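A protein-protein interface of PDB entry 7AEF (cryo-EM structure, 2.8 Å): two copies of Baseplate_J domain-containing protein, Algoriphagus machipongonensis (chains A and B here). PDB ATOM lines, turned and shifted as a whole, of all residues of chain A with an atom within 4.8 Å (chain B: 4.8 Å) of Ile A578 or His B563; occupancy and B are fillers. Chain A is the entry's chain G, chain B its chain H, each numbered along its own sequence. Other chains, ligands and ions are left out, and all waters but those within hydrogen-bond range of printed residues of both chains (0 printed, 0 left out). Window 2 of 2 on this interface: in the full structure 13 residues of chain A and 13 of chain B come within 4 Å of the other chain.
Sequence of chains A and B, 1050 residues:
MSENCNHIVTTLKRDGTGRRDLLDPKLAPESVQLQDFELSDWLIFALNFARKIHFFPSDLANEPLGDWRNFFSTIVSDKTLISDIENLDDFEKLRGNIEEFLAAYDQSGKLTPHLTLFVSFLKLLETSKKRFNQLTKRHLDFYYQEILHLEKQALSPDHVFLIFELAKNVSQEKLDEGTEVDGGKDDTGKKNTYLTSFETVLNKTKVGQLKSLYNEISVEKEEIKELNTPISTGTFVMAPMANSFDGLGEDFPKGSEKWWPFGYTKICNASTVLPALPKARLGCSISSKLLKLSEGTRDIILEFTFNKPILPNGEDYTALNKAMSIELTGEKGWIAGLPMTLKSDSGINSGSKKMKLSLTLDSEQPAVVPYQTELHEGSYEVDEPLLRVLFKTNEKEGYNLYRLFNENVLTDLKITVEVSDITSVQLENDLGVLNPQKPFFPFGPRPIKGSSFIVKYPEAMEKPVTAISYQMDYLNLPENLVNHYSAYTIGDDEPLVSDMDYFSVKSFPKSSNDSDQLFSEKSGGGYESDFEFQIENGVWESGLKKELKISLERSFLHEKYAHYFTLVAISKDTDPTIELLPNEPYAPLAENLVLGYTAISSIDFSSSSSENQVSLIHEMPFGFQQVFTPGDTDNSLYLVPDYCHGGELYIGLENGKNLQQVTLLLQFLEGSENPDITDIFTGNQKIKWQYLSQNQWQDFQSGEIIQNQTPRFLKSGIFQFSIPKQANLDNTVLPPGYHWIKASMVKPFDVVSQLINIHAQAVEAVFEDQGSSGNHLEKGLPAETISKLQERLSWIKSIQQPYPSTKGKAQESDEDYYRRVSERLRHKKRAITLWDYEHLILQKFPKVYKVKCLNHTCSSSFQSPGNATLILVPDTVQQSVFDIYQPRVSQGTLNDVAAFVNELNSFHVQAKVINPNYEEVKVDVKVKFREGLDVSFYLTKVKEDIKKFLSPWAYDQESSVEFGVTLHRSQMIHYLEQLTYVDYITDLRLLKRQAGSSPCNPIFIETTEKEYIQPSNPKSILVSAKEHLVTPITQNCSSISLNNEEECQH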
ATOM      1  N   TYR A 561      14.287   2.351 -14.536  1.00  0.00           N
ATOM      2  CA  TYR A 561      14.441   3.456 -15.479  1.00  0.00           C
ATOM      3  C   TYR A 561      13.692   3.202 -16.778  1.00  0.00           C
ATOM      4  O   TYR A 561      12.946   4.066 -17.247  1.00  0.00           O
ATOM      5  CB  TYR A 561      15.916   3.693 -15.767  1.00  0.00           C
ATOM      6  CG  TYR A 561      16.157   4.789 -16.763  1.00  0.00           C
ATOM      7  CD1 TYR A 561      15.959   6.109 -16.414  1.00  0.00           C
ATOM      8  CD2 TYR A 561      16.585   4.503 -18.044  1.00  0.00           C
ATOM      9  CE1 TYR A 561      16.180   7.111 -17.306  1.00  0.00           C
ATOM     10  CE2 TYR A 561      16.808   5.503 -18.945  1.00  0.00           C
ATOM     11  CZ  TYR A 561      16.607   6.807 -18.567  1.00  0.00           C
ATOM     12  OH  TYR A 561      16.830   7.817 -19.462  1.00  0.00           O
ATOM     13  N   PHE A 565      10.537   5.512 -18.232  1.00  0.00           N
ATOM     14  CA  PHE A 565      10.834   6.188 -19.486  1.00  0.00           C
ATOM     15  C   PHE A 565       9.787   5.865 -20.532  1.00  0.00           C
ATOM     16  O   PHE A 565       9.264   6.765 -21.197  1.00  0.00           O
ATOM     17  CB  PHE A 565      12.212   5.789 -19.998  1.00  0.00           C
ATOM     18  CG  PHE A 565      12.665   6.614 -21.149  1.00  0.00           C
ATOM     19  CD1 PHE A 565      13.338   7.793 -20.922  1.00  0.00           C
ATOM     20  CD2 PHE A 565      12.394   6.238 -22.454  1.00  0.00           C
ATOM     21  CE1 PHE A 565      13.740   8.574 -21.969  1.00  0.00           C
ATOM     22  CE2 PHE A 565      12.781   7.021 -23.499  1.00  0.00           C
ATOM     23  CZ  PHE A 565      13.461   8.189 -23.259  1.00  0.00           C
ATOM     24  N   PRO A 576       4.849  14.650 -24.047  1.00  0.00           N
ATOM     25  CA  PRO A 576       6.109  14.560 -23.296  1.00  0.00           C
ATOM     26  C   PRO A 576       6.975  15.788 -23.496  1.00  0.00           C
ATOM     27  O   PRO A 576       7.038  16.354 -24.586  1.00  0.00           O
ATOM     28  CB  PRO A 576       6.782  13.319 -23.891  1.00  0.00           C
ATOM     29  CG  PRO A 576       5.685  12.544 -24.487  1.00  0.00           C
ATOM     30  CD  PRO A 576       4.683  13.529 -24.975  1.00  0.00           C
ATOM     31  N   THR A 577       7.592  16.237 -22.413  1.00  0.00           N
ATOM     32  CA  THR A 577       8.553  17.329 -22.415  1.00  0.00           C
ATOM     33  C   THR A 577       9.783  16.802 -21.699  1.00  0.00           C
ATOM     34  O   THR A 577       9.728  15.729 -21.099  1.00  0.00           O
ATOM     35  CB  THR A 577       7.997  18.582 -21.725  1.00  0.00           C
ATOM     36  OG1 THR A 577       7.826  18.318 -20.326  1.00  0.00           O
ATOM     37  CG2 THR A 577       6.659  18.987 -22.311  1.00  0.00           C
ATOM     38  N   ILE A 578      10.897  17.542 -21.755  1.00  0.00           N
ATOM     39  CA  ILE A 578      12.121  17.045 -21.119  1.00  0.00           C
ATOM     40  C   ILE A 578      11.956  16.951 -19.602  1.00  0.00           C
ATOM     41  O   ILE A 578      12.482  16.026 -18.974  1.00  0.00           O
ATOM     42  CB  ILE A 578      13.347  17.902 -21.521  1.00  0.00           C
ATOM     43  CG1 ILE A 578      14.654  17.238 -21.071  1.00  0.00           C
ATOM     44  CG2 ILE A 578      13.281  19.315 -20.957  1.00  0.00           C
ATOM     45  CD1 ILE A 578      14.984  15.932 -21.771  1.00  0.00           C
ATOM     46  N   GLU A 579      11.125  17.816 -19.017  1.00  0.00           N
ATOM     47  CA  GLU A 579      10.903  17.850 -17.579  1.00  0.00           C
ATOM     48  C   GLU A 579      10.112  16.655 -17.077  1.00  0.00           C
ATOM     49  O   GLU A 579      10.067  16.423 -15.866  1.00  0.00           O
ATOM     50  CB  GLU A 579      10.159  19.132 -17.208  1.00  0.00           C
ATOM     51  CG  GLU A 579      10.954  20.406 -17.412  1.00  0.00           C
ATOM     52  CD  GLU A 579      10.895  20.914 -18.835  1.00  0.00           C
ATOM     53  OE1 GLU A 579      10.216  20.284 -19.669  1.00  0.00           O
ATOM     54  OE2 GLU A 579      11.546  21.929 -19.131  1.00  0.00           O
ATOM     55  N   LEU A 580       9.468  15.911 -17.967  1.00  0.00           N
ATOM     56  CA  LEU A 580       8.671  14.770 -17.567  1.00  0.00           C
ATOM     57  C   LEU A 580       9.403  13.452 -17.737  1.00  0.00           C
ATOM     58  O   LEU A 580       8.881  12.418 -17.311  1.00  0.00           O
ATOM     59  CB  LEU A 580       7.373  14.731 -18.369  1.00  0.00           C
ATOM     60  CG  LEU A 580       6.466  15.947 -18.248  1.00  0.00           C
ATOM     61  CD1 LEU A 580       5.304  15.792 -19.198  1.00  0.00           C
ATOM     62  CD2 LEU A 580       5.977  16.106 -16.826  1.00  0.00           C
ATOM     63  N   LEU A 581      10.534  13.462 -18.334  1.00  0.00           N
ATOM     64  CA  LEU A 581      11.241  12.211 -18.508  1.00  0.00           C
ATOM     65  C   LEU A 581      12.137  11.955 -17.304  1.00  0.00           C
ATOM     66  O   LEU A 581      12.646  12.895 -16.687  1.00  0.00           O
ATOM     67  CB  LEU A 581      12.072  12.240 -19.789  1.00  0.00           C
ATOM     68  CG  LEU A 581      11.286  12.276 -21.103  1.00  0.00           C
ATOM     69  CD1 LEU A 581      12.210  12.545 -22.255  1.00  0.00           C
ATOM     70  CD2 LEU A 581      10.546  10.979 -21.342  1.00  0.00           C
ATOM     71  N   PRO A 582      12.289  10.688 -16.931  1.00  0.00           N
ATOM     72  CA  PRO A 582      13.148  10.350 -15.797  1.00  0.00           C
ATOM     73  C   PRO A 582      14.609  10.580 -16.116  1.00  0.00           C
ATOM     74  O   PRO A 582      15.061  10.386 -17.245  1.00  0.00           O
ATOM     75  CB  PRO A 582      12.860   8.865 -15.573  1.00  0.00           C
ATOM     76  CG  PRO A 582      12.403   8.389 -16.895  1.00  0.00           C
ATOM     77  CD  PRO A 582      11.627   9.497 -17.485  1.00  0.00           C
ATOM     78  N   GLU A 584      18.604   9.601 -15.416  1.00  0.00           N
ATOM     79  CA  GLU A 584      19.324   8.356 -15.265  1.00  0.00           C
ATOM     80  C   GLU A 584      19.627   8.176 -13.780  1.00  0.00           C
ATOM     81  O   GLU A 584      19.990   9.149 -13.102  1.00  0.00           O
ATOM     82  CB  GLU A 584      20.597   8.526 -16.046  1.00  0.00           C
ATOM     83  CG  GLU A 584      20.332   8.275 -17.467  1.00  0.00           C
ATOM     84  CD  GLU A 584      20.285   9.680 -18.105  1.00  0.00           C
ATOM     85  OE1 GLU A 584      20.288  10.678 -17.335  1.00  0.00           O
ATOM     86  OE2 GLU A 584      20.157   9.818 -19.328  1.00  0.00           O
ATOM     87  N   THR B 489      18.083  22.460 -25.314  1.00  0.00           N
ATOM     88  CA  THR B 489      17.513  23.612 -24.630  1.00  0.00           C
ATOM     89  C   THR B 489      16.603  23.177 -23.492  1.00  0.00           C
ATOM     90  O   THR B 489      16.118  22.047 -23.460  1.00  0.00           O
ATOM     91  CB  THR B 489      16.702  24.479 -25.587  1.00  0.00           C
ATOM     92  OG1 THR B 489      15.569  23.739 -26.046  1.00  0.00           O
ATOM     93  CG2 THR B 489      17.523  24.886 -26.784  1.00  0.00           C
ATOM     94  N   GLU B 559      25.008  12.365 -21.573  1.00  0.00           N
ATOM     95  CA  GLU B 559      23.857  11.806 -20.887  1.00  0.00           C
ATOM     96  C   GLU B 559      22.511  12.347 -21.371  1.00  0.00           C
ATOM     97  O   GLU B 559      21.477  11.811 -20.964  1.00  0.00           O
ATOM     98  CB  GLU B 559      24.027  12.065 -19.386  1.00  0.00           C
ATOM     99  CG  GLU B 559      24.052  13.546 -18.964  1.00  0.00           C
ATOM    100  CD  GLU B 559      25.428  14.190 -19.037  1.00  0.00           C
ATOM    101  OE1 GLU B 559      26.313  13.639 -19.702  1.00  0.00           O
ATOM    102  OE2 GLU B 559      25.626  15.259 -18.440  1.00  0.00           O
ATOM    103  N   LYS B 560      22.476  13.384 -22.208  1.00  0.00           N
ATOM    104  CA  LYS B 560      21.210  13.931 -22.668  1.00  0.00           C
ATOM    105  C   LYS B 560      20.886  13.651 -24.120  1.00  0.00           C
ATOM    106  O   LYS B 560      19.783  14.000 -24.542  1.00  0.00           O
ATOM    107  CB  LYS B 560      21.167  15.452 -22.495  1.00  0.00           C
ATOM    108  CG  LYS B 560      21.283  15.947 -21.093  1.00  0.00           C
ATOM    109  CD  LYS B 560      20.122  15.492 -20.254  1.00  0.00           C
ATOM    110  CE  LYS B 560      20.153  16.137 -18.894  1.00  0.00           C
ATOM    111  NZ  LYS B 560      19.029  15.662 -18.039  1.00  0.00           N
ATOM    112  N   TYR B 561      21.808  13.077 -24.890  1.00  0.00           N
ATOM    113  CA  TYR B 561      21.597  12.953 -26.329  1.00  0.00           C
ATOM    114  C   TYR B 561      20.338  12.164 -26.662  1.00  0.00           C
ATOM    115  O   TYR B 561      19.514  12.616 -27.458  1.00  0.00           O
ATOM    116  CB  TYR B 561      22.802  12.298 -26.972  1.00  0.00           C
ATOM    117  CG  TYR B 561      22.658  12.098 -28.443  1.00  0.00           C
ATOM    118  CD1 TYR B 561      22.744  13.168 -29.305  1.00  0.00           C
ATOM    119  CD2 TYR B 561      22.458  10.843 -28.972  1.00  0.00           C
ATOM    120  CE1 TYR B 561      22.638  13.003 -30.641  1.00  0.00           C
ATOM    121  CE2 TYR B 561      22.349  10.667 -30.320  1.00  0.00           C
ATOM    122  CZ  TYR B 561      22.442  11.756 -31.147  1.00  0.00           C
ATOM    123  OH  TYR B 561      22.332  11.596 -32.499  1.00  0.00           O
ATOM    124  N   ALA B 562      20.144  11.027 -25.996  1.00  0.00           N
ATOM    125  CA  ALA B 562      19.005  10.160 -26.283  1.00  0.00           C
ATOM    126  C   ALA B 562      17.673  10.837 -26.012  1.00  0.00           C
ATOM    127  O   ALA B 562      16.700  10.621 -26.739  1.00  0.00           O
ATOM    128  CB  ALA B 562      19.101   8.907 -25.434  1.00  0.00           C
ATOM    129  N   HIS B 563      17.616  11.620 -24.941  1.00  0.00           N
ATOM    130  CA  HIS B 563      16.412  12.337 -24.545  1.00  0.00           C
ATOM    131  C   HIS B 563      16.006  13.410 -25.540  1.00  0.00           C
ATOM    132  O   HIS B 563      14.826  13.556 -25.830  1.00  0.00           O
ATOM    133  CB  HIS B 563      16.631  12.997 -23.200  1.00  0.00           C
ATOM    134  CG  HIS B 563      16.749  12.038 -22.065  1.00  0.00           C
ATOM    135  ND1 HIS B 563      16.088  12.227 -20.875  1.00  0.00           N
ATOM    136  CD2 HIS B 563      17.457  10.895 -21.929  1.00  0.00           C
ATOM    137  CE1 HIS B 563      16.377  11.234 -20.054  1.00  0.00           C
ATOM    138  NE2 HIS B 563      17.207  10.413 -20.670  1.00  0.00           N
ATOM    139  N   TYR B 564      16.950  14.198 -26.032  1.00  0.00           N
ATOM    140  CA  TYR B 564      16.599  15.251 -26.970  1.00  0.00           C
ATOM    141  C   TYR B 564      16.298  14.686 -28.335  1.00  0.00           C
ATOM    142  O   TYR B 564      15.383  15.168 -29.007  1.00  0.00           O
ATOM    143  CB  TYR B 564      17.722  16.270 -27.059  1.00  0.00           C
ATOM    144  CG  TYR B 564      17.720  17.228 -25.917  1.00  0.00           C
ATOM    145  CD1 TYR B 564      16.734  18.178 -25.812  1.00  0.00           C
ATOM    146  CD2 TYR B 564      18.696  17.180 -24.945  1.00  0.00           C
ATOM    147  CE1 TYR B 564      16.718  19.062 -24.783  1.00  0.00           C
ATOM    148  CE2 TYR B 564      18.687  18.068 -23.899  1.00  0.00           C
ATOM    149  CZ  TYR B 564      17.692  19.007 -23.829  1.00  0.00           C
ATOM    150  OH  TYR B 564      17.664  19.909 -22.800  1.00  0.00           O
ATOM    151  N   PHE B 565      17.045  13.657 -28.736  1.00  0.00           N
ATOM    152  CA  PHE B 565      16.818  13.029 -30.027  1.00  0.00           C
ATOM    153  C   PHE B 565      15.402  12.506 -30.123  1.00  0.00           C
ATOM    154  O   PHE B 565      14.700  12.767 -31.107  1.00  0.00           O
ATOM    155  CB  PHE B 565      17.798  11.887 -30.240  1.00  0.00           C
ATOM    156  CG  PHE B 565      17.756  11.343 -31.610  1.00  0.00           C
ATOM    157  CD1 PHE B 565      18.541  11.901 -32.586  1.00  0.00           C
ATOM    158  CD2 PHE B 565      16.916  10.299 -31.948  1.00  0.00           C
ATOM    159  CE1 PHE B 565      18.505  11.432 -33.866  1.00  0.00           C
ATOM    160  CE2 PHE B 565      16.866   9.839 -33.228  1.00  0.00           C
ATOM    161  CZ  PHE B 565      17.665  10.402 -34.189  1.00  0.00           C
ATOM    162  N   THR B 566      14.968  11.804 -29.074  1.00  0.00           N
ATOM    163  CA  THR B 566      13.636  11.222 -29.022  1.00  0.00           C
ATOM    164  C   THR B 566      12.558  12.280 -29.124  1.00  0.00           C
ATOM    165  O   THR B 566      11.621  12.131 -29.910  1.00  0.00           O
ATOM    166  CB  THR B 566      13.437  10.449 -27.722  1.00  0.00           C
ATOM    167  OG1 THR B 566      14.371   9.373 -27.645  1.00  0.00           O
ATOM    168  CG2 THR B 566      12.020   9.891 -27.659  1.00  0.00           C
ATOM    169  N   LEU B 567      12.683  13.359 -28.345  1.00  0.00           N
ATOM    170  CA  LEU B 567      11.639  14.376 -28.304  1.00  0.00           C
ATOM    171  C   LEU B 567      11.434  15.039 -29.645  1.00  0.00           C
ATOM    172  O   LEU B 567      10.298  15.349 -30.013  1.00  0.00           O
ATOM    173  CB  LEU B 567      11.974  15.446 -27.286  1.00  0.00           C
ATOM    174  CG  LEU B 567      11.892  15.059 -25.827  1.00  0.00           C
ATOM    175  CD1 LEU B 567      12.456  16.194 -25.009  1.00  0.00           C
ATOM    176  CD2 LEU B 567      10.461  14.760 -25.433  1.00  0.00           C
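Of the printed residues of chain B, Tyr A561 touches His B563 (2.9 Å). Of the printed residues of chain B, Pro A576 touches Leu B567 (3.9 Å). Ile A578 touches just these residues of chain B: His B563 and Leu B567. Of the printed residues of chain A, Glu B559 touches Glu A584 (2.9 Å). His B563 touches just these residues of chain A: Tyr A561 (2.9 Å), Ile A578 (3.7 Å), Pro A582 (3.2 Å) and Glu A584 (3.3 Å). Printed residues of chain A within 4 Å of Leu B567: Pro A576 and Ile A578. The nearest residue of chain B that does not touch Ile A578 is Tyr B564 (4.4 Å). The nearest printed residue of chain A that does not touch His B563 is Leu A581 (4.1 Å).
Among the printed residues, merely in contact across the chains: Pro A582 with His B563, Ile A578 with His B563, Ile A578 with Leu B567 and Pro A576 with Leu B567.
Positions printed for both chains: 561 and 565. Of the 7 pairs that touch across the chains among the printed residues, none has its exchanged pair printed and touching as well.
The side-chain carboxylate (OE2) of Glu A584 is in hydrogen-bond range of a ring nitrogen (NE2) of His B563 (3.3 Å). The backbone carbonyl oxygen of Glu B559 lies close to the side-chain carboxylate of Glu A584 (2.9 Å). The side-chain hydroxyl (OH) of Tyr A561 is in hydrogen-bond range of a ring nitrogen (NE2) of His B563, 2.9 Å away.
Hydrophobic or aromatic side chains of chain A that line the printed part of chain B: Tyr A561 and Ile A578. Of the 10 printed residues of chain B, 3 touch a printed residue of chain A. Among the printed residues, 7 pairs touch across the chains.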
